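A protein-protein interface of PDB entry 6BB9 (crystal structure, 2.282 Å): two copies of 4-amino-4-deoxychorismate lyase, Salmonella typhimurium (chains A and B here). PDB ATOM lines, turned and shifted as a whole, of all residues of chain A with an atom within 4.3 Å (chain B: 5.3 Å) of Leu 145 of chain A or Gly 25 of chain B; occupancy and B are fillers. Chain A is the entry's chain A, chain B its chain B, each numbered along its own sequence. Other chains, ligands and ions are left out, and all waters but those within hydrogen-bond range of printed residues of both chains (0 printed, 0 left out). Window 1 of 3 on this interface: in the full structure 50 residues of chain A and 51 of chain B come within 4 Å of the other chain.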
ATOM      1  N   ALA A  21     -34.690 -27.687  25.520  1.00  0.00           N
ATOM      2  CA  ALA A  21     -33.439 -27.230  24.930  1.00  0.00           C
ATOM      3  C   ALA A  21     -32.547 -28.420  24.623  1.00  0.00           C
ATOM      4  O   ALA A  21     -31.979 -28.523  23.529  1.00  0.00           O
ATOM      5  CB  ALA A  21     -32.729 -26.252  25.859  1.00  0.00           C
ATOM      6  N   GLY A  25     -33.423 -28.438  20.971  1.00  0.00           N
ATOM      7  CA  GLY A  25     -32.980 -27.069  20.793  1.00  0.00           C
ATOM      8  C   GLY A  25     -34.127 -26.087  20.825  1.00  0.00           C
ATOM      9  O   GLY A  25     -34.093 -25.068  20.122  1.00  0.00           O
ATOM     10  N   GLY A  27     -35.558 -23.367  21.900  1.00  0.00           N
ATOM     11  CA  GLY A  27     -35.445 -22.065  22.523  1.00  0.00           C
ATOM     12  C   GLY A  27     -34.450 -21.201  21.772  1.00  0.00           C
ATOM     13  O   GLY A  27     -34.114 -21.471  20.611  1.00  0.00           O
ATOM     14  N   SER A  28     -33.985 -20.156  22.459  1.00  0.00           N
ATOM     15  CA  SER A  28     -33.074 -19.191  21.861  1.00  0.00           C
ATOM     16  C   SER A  28     -32.119 -18.651  22.915  1.00  0.00           C
ATOM     17  O   SER A  28     -32.244 -18.940  24.112  1.00  0.00           O
ATOM     18  CB  SER A  28     -33.841 -18.046  21.195  1.00  0.00           C
ATOM     19  OG  SER A  28     -34.328 -17.136  22.164  1.00  0.00           O
ATOM     20  N   PHE A  29     -31.148 -17.859  22.458  1.00  0.00           N
ATOM     21  CA  PHE A  29     -30.136 -17.336  23.364  1.00  0.00           C
ATOM     22  C   PHE A  29     -29.588 -16.000  22.875  1.00  0.00           C
ATOM     23  O   PHE A  29     -29.941 -15.489  21.806  1.00  0.00           O
ATOM     24  CB  PHE A  29     -28.993 -18.343  23.581  1.00  0.00           C
ATOM     25  CG  PHE A  29     -28.097 -18.560  22.381  1.00  0.00           C
ATOM     26  CD1 PHE A  29     -28.525 -19.336  21.297  1.00  0.00           C
ATOM     27  CD2 PHE A  29     -26.803 -18.056  22.368  1.00  0.00           C
ATOM     28  CE1 PHE A  29     -27.689 -19.571  20.200  1.00  0.00           C
ATOM     29  CE2 PHE A  29     -25.953 -18.285  21.279  1.00  0.00           C
ATOM     30  CZ  PHE A  29     -26.400 -19.040  20.185  1.00  0.00           C
ATOM     31  N   ILE A  85     -29.896 -18.190  28.033  1.00  0.00           N
ATOM     32  CA  ILE A  85     -30.727 -19.104  27.252  1.00  0.00           C
ATOM     33  C   ILE A  85     -32.141 -19.096  27.824  1.00  0.00           C
ATOM     34  O   ILE A  85     -32.327 -19.244  29.038  1.00  0.00           O
ATOM     35  CB  ILE A  85     -30.170 -20.540  27.254  1.00  0.00           C
ATOM     36  CG1 ILE A  85     -28.807 -20.596  26.589  1.00  0.00           C
ATOM     37  CG2 ILE A  85     -31.155 -21.507  26.560  1.00  0.00           C
ATOM     38  CD1 ILE A  85     -28.149 -21.948  26.722  1.00  0.00           C
ATOM     39  N   LYS A 143     -31.439 -15.853  16.882  1.00  0.00           N
ATOM     40  CA  LYS A 143     -30.368 -16.617  17.519  1.00  0.00           C
ATOM     41  C   LYS A 143     -30.971 -17.778  18.317  1.00  0.00           C
ATOM     42  O   LYS A 143     -30.878 -17.850  19.543  1.00  0.00           O
ATOM     43  CB  LYS A 143     -29.522 -15.707  18.403  1.00  0.00           C
ATOM     44  CG  LYS A 143     -28.101 -16.197  18.615  1.00  0.00           C
ATOM     45  CD  LYS A 143     -27.383 -15.346  19.629  1.00  0.00           C
ATOM     46  CE  LYS A 143     -25.884 -15.403  19.432  1.00  0.00           C
ATOM     47  NZ  LYS A 143     -25.388 -14.137  18.840  1.00  0.00           N
ATOM     48  N   HIS A 144     -31.617 -18.695  17.595  1.00  0.00           N
ATOM     49  CA  HIS A 144     -32.196 -19.859  18.247  1.00  0.00           C
ATOM     50  C   HIS A 144     -31.115 -20.896  18.535  1.00  0.00           C
ATOM     51  O   HIS A 144     -29.965 -20.770  18.114  1.00  0.00           O
ATOM     52  CB  HIS A 144     -33.320 -20.452  17.400  1.00  0.00           C
ATOM     53  CG  HIS A 144     -32.911 -20.791  16.007  1.00  0.00           C
ATOM     54  ND1 HIS A 144     -32.121 -21.881  15.707  1.00  0.00           N
ATOM     55  CD2 HIS A 144     -33.178 -20.179  14.826  1.00  0.00           C
ATOM     56  CE1 HIS A 144     -31.920 -21.927  14.400  1.00  0.00           C
ATOM     57  NE2 HIS A 144     -32.551 -20.905  13.844  1.00  0.00           N
ATOM     58  N   LEU A 145     -31.495 -21.927  19.286  1.00  0.00           N
ATOM     59  CA  LEU A 145     -30.548 -22.930  19.762  1.00  0.00           C
ATOM     60  C   LEU A 145     -30.204 -23.987  18.714  1.00  0.00           C
ATOM     61  O   LEU A 145     -29.287 -24.780  18.949  1.00  0.00           O
ATOM     62  CB  LEU A 145     -31.095 -23.636  21.023  1.00  0.00           C
ATOM     63  CG  LEU A 145     -31.268 -22.868  22.346  1.00  0.00           C
ATOM     64  CD1 LEU A 145     -32.007 -23.720  23.388  1.00  0.00           C
ATOM     65  CD2 LEU A 145     -29.928 -22.406  22.910  1.00  0.00           C
ATOM     66  N   ASN A 146     -30.921 -24.043  17.587  1.00  0.00           N
ATOM     67  CA  ASN A 146     -30.631 -25.012  16.518  1.00  0.00           C
ATOM     68  C   ASN A 146     -29.420 -24.506  15.736  1.00  0.00           C
ATOM     69  O   ASN A 146     -29.535 -23.889  14.675  1.00  0.00           O
ATOM     70  CB  ASN A 146     -31.840 -25.206  15.598  1.00  0.00           C
ATOM     71  CG  ASN A 146     -32.904 -26.132  16.183  1.00  0.00           C
ATOM     72  OD1 ASN A 146     -33.638 -26.777  15.442  1.00  0.00           O
ATOM     73  ND2 ASN A 146     -32.994 -26.197  17.513  1.00  0.00           N
ATOM     74  N   ARG A 147     -28.230 -24.775  16.278  1.00  0.00           N
ATOM     75  CA  ARG A 147     -26.991 -24.206  15.759  1.00  0.00           C
ATOM     76  C   ARG A 147     -26.085 -25.257  15.133  1.00  0.00           C
ATOM     77  O   ARG A 147     -24.901 -24.993  14.902  1.00  0.00           O
ATOM     78  CB  ARG A 147     -26.245 -23.453  16.866  1.00  0.00           C
ATOM     79  CG  ARG A 147     -26.857 -22.091  17.216  1.00  0.00           C
ATOM     80  CD  ARG A 147     -26.917 -21.209  15.979  1.00  0.00           C
ATOM     81  NE  ARG A 147     -28.115 -20.390  15.975  1.00  0.00           N
ATOM     82  CZ  ARG A 147     -28.777 -20.023  14.887  1.00  0.00           C
ATOM     83  NH1 ARG A 147     -28.369 -20.401  13.683  1.00  0.00           N
ATOM     84  NH2 ARG A 147     -29.862 -19.279  15.011  1.00  0.00           N
ATOM     85  N   LEU A 148     -26.618 -26.439  14.839  1.00  0.00           N
ATOM     86  CA  LEU A 148     -25.776 -27.496  14.296  1.00  0.00           C
ATOM     87  C   LEU A 148     -25.090 -27.050  13.012  1.00  0.00           C
ATOM     88  O   LEU A 148     -23.939 -27.426  12.766  1.00  0.00           O
ATOM     89  CB  LEU A 148     -26.609 -28.756  14.066  1.00  0.00           C
ATOM     90  CG  LEU A 148     -25.903 -30.114  14.055  1.00  0.00           C
ATOM     91  CD1 LEU A 148     -24.781 -30.188  15.078  1.00  0.00           C
ATOM     92  CD2 LEU A 148     -26.927 -31.218  14.313  1.00  0.00           C
ATOM     93  N   ARG B  20     -23.484 -29.830  24.964  1.00  0.00           N
ATOM     94  CA  ARG B  20     -23.754 -29.148  23.708  1.00  0.00           C
ATOM     95  C   ARG B  20     -25.088 -29.552  23.082  1.00  0.00           C
ATOM     96  O   ARG B  20     -25.527 -28.896  22.129  1.00  0.00           O
ATOM     97  CB  ARG B  20     -22.569 -29.368  22.763  1.00  0.00           C
ATOM     98  CG  ARG B  20     -21.309 -28.618  23.240  1.00  0.00           C
ATOM     99  CD  ARG B  20     -20.057 -29.008  22.480  1.00  0.00           C
ATOM    100  NE  ARG B  20     -20.185 -28.710  21.060  1.00  0.00           N
ATOM    101  CZ  ARG B  20     -19.550 -27.727  20.429  1.00  0.00           C
ATOM    102  NH1 ARG B  20     -18.714 -26.932  21.089  1.00  0.00           N
ATOM    103  NH2 ARG B  20     -19.750 -27.544  19.130  1.00  0.00           N
ATOM    104  N   ALA B  21     -25.759 -30.584  23.602  1.00  0.00           N
ATOM    105  CA  ALA B  21     -27.159 -30.792  23.236  1.00  0.00           C
ATOM    106  C   ALA B  21     -28.016 -29.630  23.715  1.00  0.00           C
ATOM    107  O   ALA B  21     -28.902 -29.155  22.996  1.00  0.00           O
ATOM    108  CB  ALA B  21     -27.677 -32.101  23.831  1.00  0.00           C
ATOM    109  N   THR B  22     -27.764 -29.176  24.941  1.00  0.00           N
ATOM    110  CA  THR B  22     -28.485 -28.049  25.514  1.00  0.00           C
ATOM    111  C   THR B  22     -28.091 -26.739  24.846  1.00  0.00           C
ATOM    112  O   THR B  22     -28.939 -25.867  24.632  1.00  0.00           O
ATOM    113  CB  THR B  22     -28.200 -27.999  27.013  1.00  0.00           C
ATOM    114  OG1 THR B  22     -28.565 -29.257  27.595  1.00  0.00           O
ATOM    115  CG2 THR B  22     -28.959 -26.862  27.692  1.00  0.00           C
ATOM    116  N   GLN B  23     -26.813 -26.582  24.501  1.00  0.00           N
ATOM    117  CA  GLN B  23     -26.355 -25.303  23.963  1.00  0.00           C
ATOM    118  C   GLN B  23     -26.708 -25.154  22.483  1.00  0.00           C
ATOM    119  O   GLN B  23     -27.202 -24.105  22.061  1.00  0.00           O
ATOM    120  CB  GLN B  23     -24.845 -25.162  24.170  1.00  0.00           C
ATOM    121  CG  GLN B  23     -24.398 -25.326  25.617  1.00  0.00           C
ATOM    122  CD  GLN B  23     -24.790 -24.148  26.485  1.00  0.00           C
ATOM    123  OE1 GLN B  23     -24.765 -23.000  26.040  1.00  0.00           O
ATOM    124  NE2 GLN B  23     -25.156 -24.424  27.733  1.00  0.00           N
ATOM    125  N   PHE B  24     -26.467 -26.196  21.682  1.00  0.00           N
ATOM    126  CA  PHE B  24     -26.549 -26.092  20.236  1.00  0.00           C
ATOM    127  C   PHE B  24     -27.399 -27.179  19.591  1.00  0.00           C
ATOM    128  O   PHE B  24     -27.452 -27.243  18.355  1.00  0.00           O
ATOM    129  CB  PHE B  24     -25.141 -26.141  19.611  1.00  0.00           C
ATOM    130  CG  PHE B  24     -24.153 -25.165  20.218  1.00  0.00           C
ATOM    131  CD1 PHE B  24     -24.461 -23.814  20.327  1.00  0.00           C
ATOM    132  CD2 PHE B  24     -22.916 -25.608  20.675  1.00  0.00           C
ATOM    133  CE1 PHE B  24     -23.547 -22.919  20.872  1.00  0.00           C
ATOM    134  CE2 PHE B  24     -22.003 -24.730  21.229  1.00  0.00           C
ATOM    135  CZ  PHE B  24     -22.318 -23.376  21.329  1.00  0.00           C
ATOM    136  N   GLY B  25     -28.059 -28.028  20.374  1.00  0.00           N
ATOM    137  CA  GLY B  25     -28.655 -29.229  19.802  1.00  0.00           C
ATOM    138  C   GLY B  25     -27.633 -30.090  19.088  1.00  0.00           C
ATOM    139  O   GLY B  25     -27.940 -30.698  18.052  1.00  0.00           O
ATOM    140  N   ASP B  26     -26.411 -30.144  19.622  1.00  0.00           N
ATOM    141  CA  ASP B  26     -25.261 -30.763  18.958  1.00  0.00           C
ATOM    142  C   ASP B  26     -25.290 -32.265  19.222  1.00  0.00           C
ATOM    143  O   ASP B  26     -24.573 -32.799  20.070  1.00  0.00           O
ATOM    144  CB  ASP B  26     -23.972 -30.126  19.461  1.00  0.00           C
ATOM    145  CG  ASP B  26     -22.767 -30.476  18.617  1.00  0.00           C
ATOM    146  OD1 ASP B  26     -22.918 -31.234  17.630  1.00  0.00           O
ATOM    147  OD2 ASP B  26     -21.657 -29.983  18.952  1.00  0.00           O
ATOM    148  N   GLY B  27     -26.136 -32.957  18.470  1.00  0.00           N
ATOM    149  CA  GLY B  27     -26.242 -34.394  18.611  1.00  0.00           C
ATOM    150  C   GLY B  27     -27.412 -34.925  17.809  1.00  0.00           C
ATOM    151  O   GLY B  27     -27.979 -34.228  16.968  1.00  0.00           O
ATOM    152  N   LEU B 145     -30.711 -33.388  16.614  1.00  0.00           N
ATOM    153  CA  LEU B 145     -31.413 -32.701  17.696  1.00  0.00           C
ATOM    154  C   LEU B 145     -31.950 -31.328  17.306  1.00  0.00           C
ATOM    155  O   LEU B 145     -32.693 -30.736  18.093  1.00  0.00           O
ATOM    156  CB  LEU B 145     -30.498 -32.537  18.917  1.00  0.00           C
ATOM    157  CG  LEU B 145     -30.084 -33.798  19.665  1.00  0.00           C
ATOM    158  CD1 LEU B 145     -29.025 -33.467  20.691  1.00  0.00           C
ATOM    159  CD2 LEU B 145     -31.275 -34.445  20.330  1.00  0.00           C
ATOM    160  N   ASN B 146     -31.598 -30.801  16.132  1.00  0.00           N
ATOM    161  CA  ASN B 146     -32.076 -29.486  15.703  1.00  0.00           C
ATOM    162  C   ASN B 146     -33.471 -29.659  15.113  1.00  0.00           C
ATOM    163  O   ASN B 146     -33.665 -29.748  13.899  1.00  0.00           O
ATOM    164  CB  ASN B 146     -31.117 -28.862  14.695  1.00  0.00           C
ATOM    165  CG  ASN B 146     -29.910 -28.219  15.352  1.00  0.00           C
ATOM    166  OD1 ASN B 146     -29.332 -27.289  14.805  1.00  0.00           O
ATOM    167  ND2 ASN B 146     -29.537 -28.700  16.537  1.00  0.00           N
ATOM    168  N   LEU B 148     -36.343 -27.678  15.871  1.00  0.00           N
ATOM    169  CA  LEU B 148     -37.255 -26.541  15.998  1.00  0.00           C
ATOM    170  C   LEU B 148     -38.260 -26.468  14.851  1.00  0.00           C
ATOM    171  O   LEU B 148     -39.386 -25.984  15.043  1.00  0.00           O
ATOM    172  CB  LEU B 148     -36.469 -25.231  16.079  1.00  0.00           C
ATOM    173  CG  LEU B 148     -36.395 -24.566  17.458  1.00  0.00           C
ATOM    174  CD1 LEU B 148     -35.596 -23.265  17.389  1.00  0.00           C
ATOM    175  CD2 LEU B 148     -37.795 -24.315  18.020  1.00  0.00           C
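The side-chain amide oxygen (OD1) of Asn 146 of chain A lies close to the backbone carbonyl oxygen (O) of Asn 146 of chain B (3.3 Å).
The side-chain amide oxygen (OD1) of Asn 146 of chain A lies within hydrogen-bond range of the backbone NH (N) of Leu 148 of chain B (2.9 Å).
O of Phe 24 of chain B lies within hydrogen-bond range of N of Arg 147 of chain A (3.3 Å).
N of Arg 147 of chain A sits at hydrogen-bond distance from OD1 of Asn 146 of chain B (3.1 Å).
The backbone NH (N) of Leu 148 of chain A lies within hydrogen-bond range of the side-chain amide oxygen (OD1) of Asn 146 of chain B, at 2.8 Å.
O of Ala 21 of chain A lies close to O of Ala 21 of chain B.
The backbone carbonyl oxygen (O) of Leu 145 of chain A sits close to the backbone carbonyl oxygen (O) of Phe 24 of chain B (3.1 Å).
The backbone carbonyl oxygen of Gly 27 of chain A is in hydrogen-bond range of the backbone NH of Leu 145 of chain A, 3.0 Å away.
The guanidinium group (NE) of Arg 147 of chain A is in hydrogen-bond range of the backbone carbonyl oxygen (O) of His 144 of chain A (2.9 Å).
N of Gly 25 of chain B lies within hydrogen-bond range of O of Arg 20 of chain B, 3.2 Å away.
The backbone carbonyl oxygen (O) of Phe 24 of chain B lies within hydrogen-bond range of the side-chain amide nitrogen (ND2) of Asn 146 of chain B, at 3.1 Å.
O of Gly 25 of chain B sits at hydrogen-bond distance from ND2 of Asn 146 of chain B (3.0 Å).
N of Leu 145 of chain B lies within hydrogen-bond range of O of Gly 27 of chain B.
N of Gly 25 of chain A touches O of Leu 145 of chain B, 3.8 Å away.
Leu 148 of chain B touches Gly 25 of chain A.
O of Gly 27 of chain A touches CD1 of Leu 148 of chain B, 3.97 Å away.
Ile 85 of chain A touches Gln 23 of chain B.
Leu 145 of chain A touches Thr 22 of chain B (CD1 to O, 3.9 Å).
CD2 of Leu 145 of chain A touches O of Gln 23 of chain B, 3.3 Å away.
Gly 25 of chain B touches Leu 145 of chain A (N to O, 3.8 Å).
Leu 148 of chain A touches Phe 24 of chain B (N to O, 3.7 Å).
CD2 of Leu 148 of chain A touches O of Gly 25 of chain B, at 3.9 Å.
Asp 26 of chain B touches Leu 148 of chain A.
Leu 145 of chain A touches four residues of chain B.
Of chain A, only Leu 145 (3.8 Å) and Leu 148 (3.9 Å) come within 4 Å of Gly 25 of chain B.
Printed residues of chain A within 4 Å of Leu 145 of chain B: Gly 25.
Of the printed residues of chain A, Ala 21 of chain B touches Ala 21 (3.2 Å).
Of the printed residues of chain A, Asn 146 of chain B touches Asn 146, Arg 147 and Leu 148.
Of the printed residues of chain B, Gly 27 of chain A touches Leu 148.
Lys 143 of chain A touches none of the printed residues of chain B.
Gly 27 of chain B touches none of the printed residues of chain A.
The nearest printed residue of chain A that does not touch Gly 25 of chain B is Gly 25 of chain A (4.9 Å).
Of the 12 printed residues of chain A, 9 touch a printed residue of chain B.
Printed residues of chain B that touch a printed residue of chain A: Ala 21, Thr 22, Gln 23, Phe 24, Gly 25, Asp 26, Leu 145, Asn 146 and Leu 148.
Among the printed residues, 18 pairs touch across the chains.
Among the printed residues, no Asp or Glu carboxylate lies within 4 Å of a Lys or Arg side-chain nitrogen of the other chain.
Ala 21 of chain B touches its own counterpart, Ala 21 of chain A.
Gly 25 of chain A touches Leu 145 of chain B, and with the chains exchanged Leu 145 of chain A touches Gly 25 of chain B.
Gly 27 of chain A touches Leu 148 of chain B, but with the chains exchanged Leu 148 of chain A does not touch Gly 27 of chain B (4.1 Å).
Asn 146 of chain A touches its own counterpart, Asn 146 of chain B.
6 positions are printed for both chains.
Of the 18 pairs that touch across the chains among the printed residues, 8 have their exchanged pair printed and touching as well.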
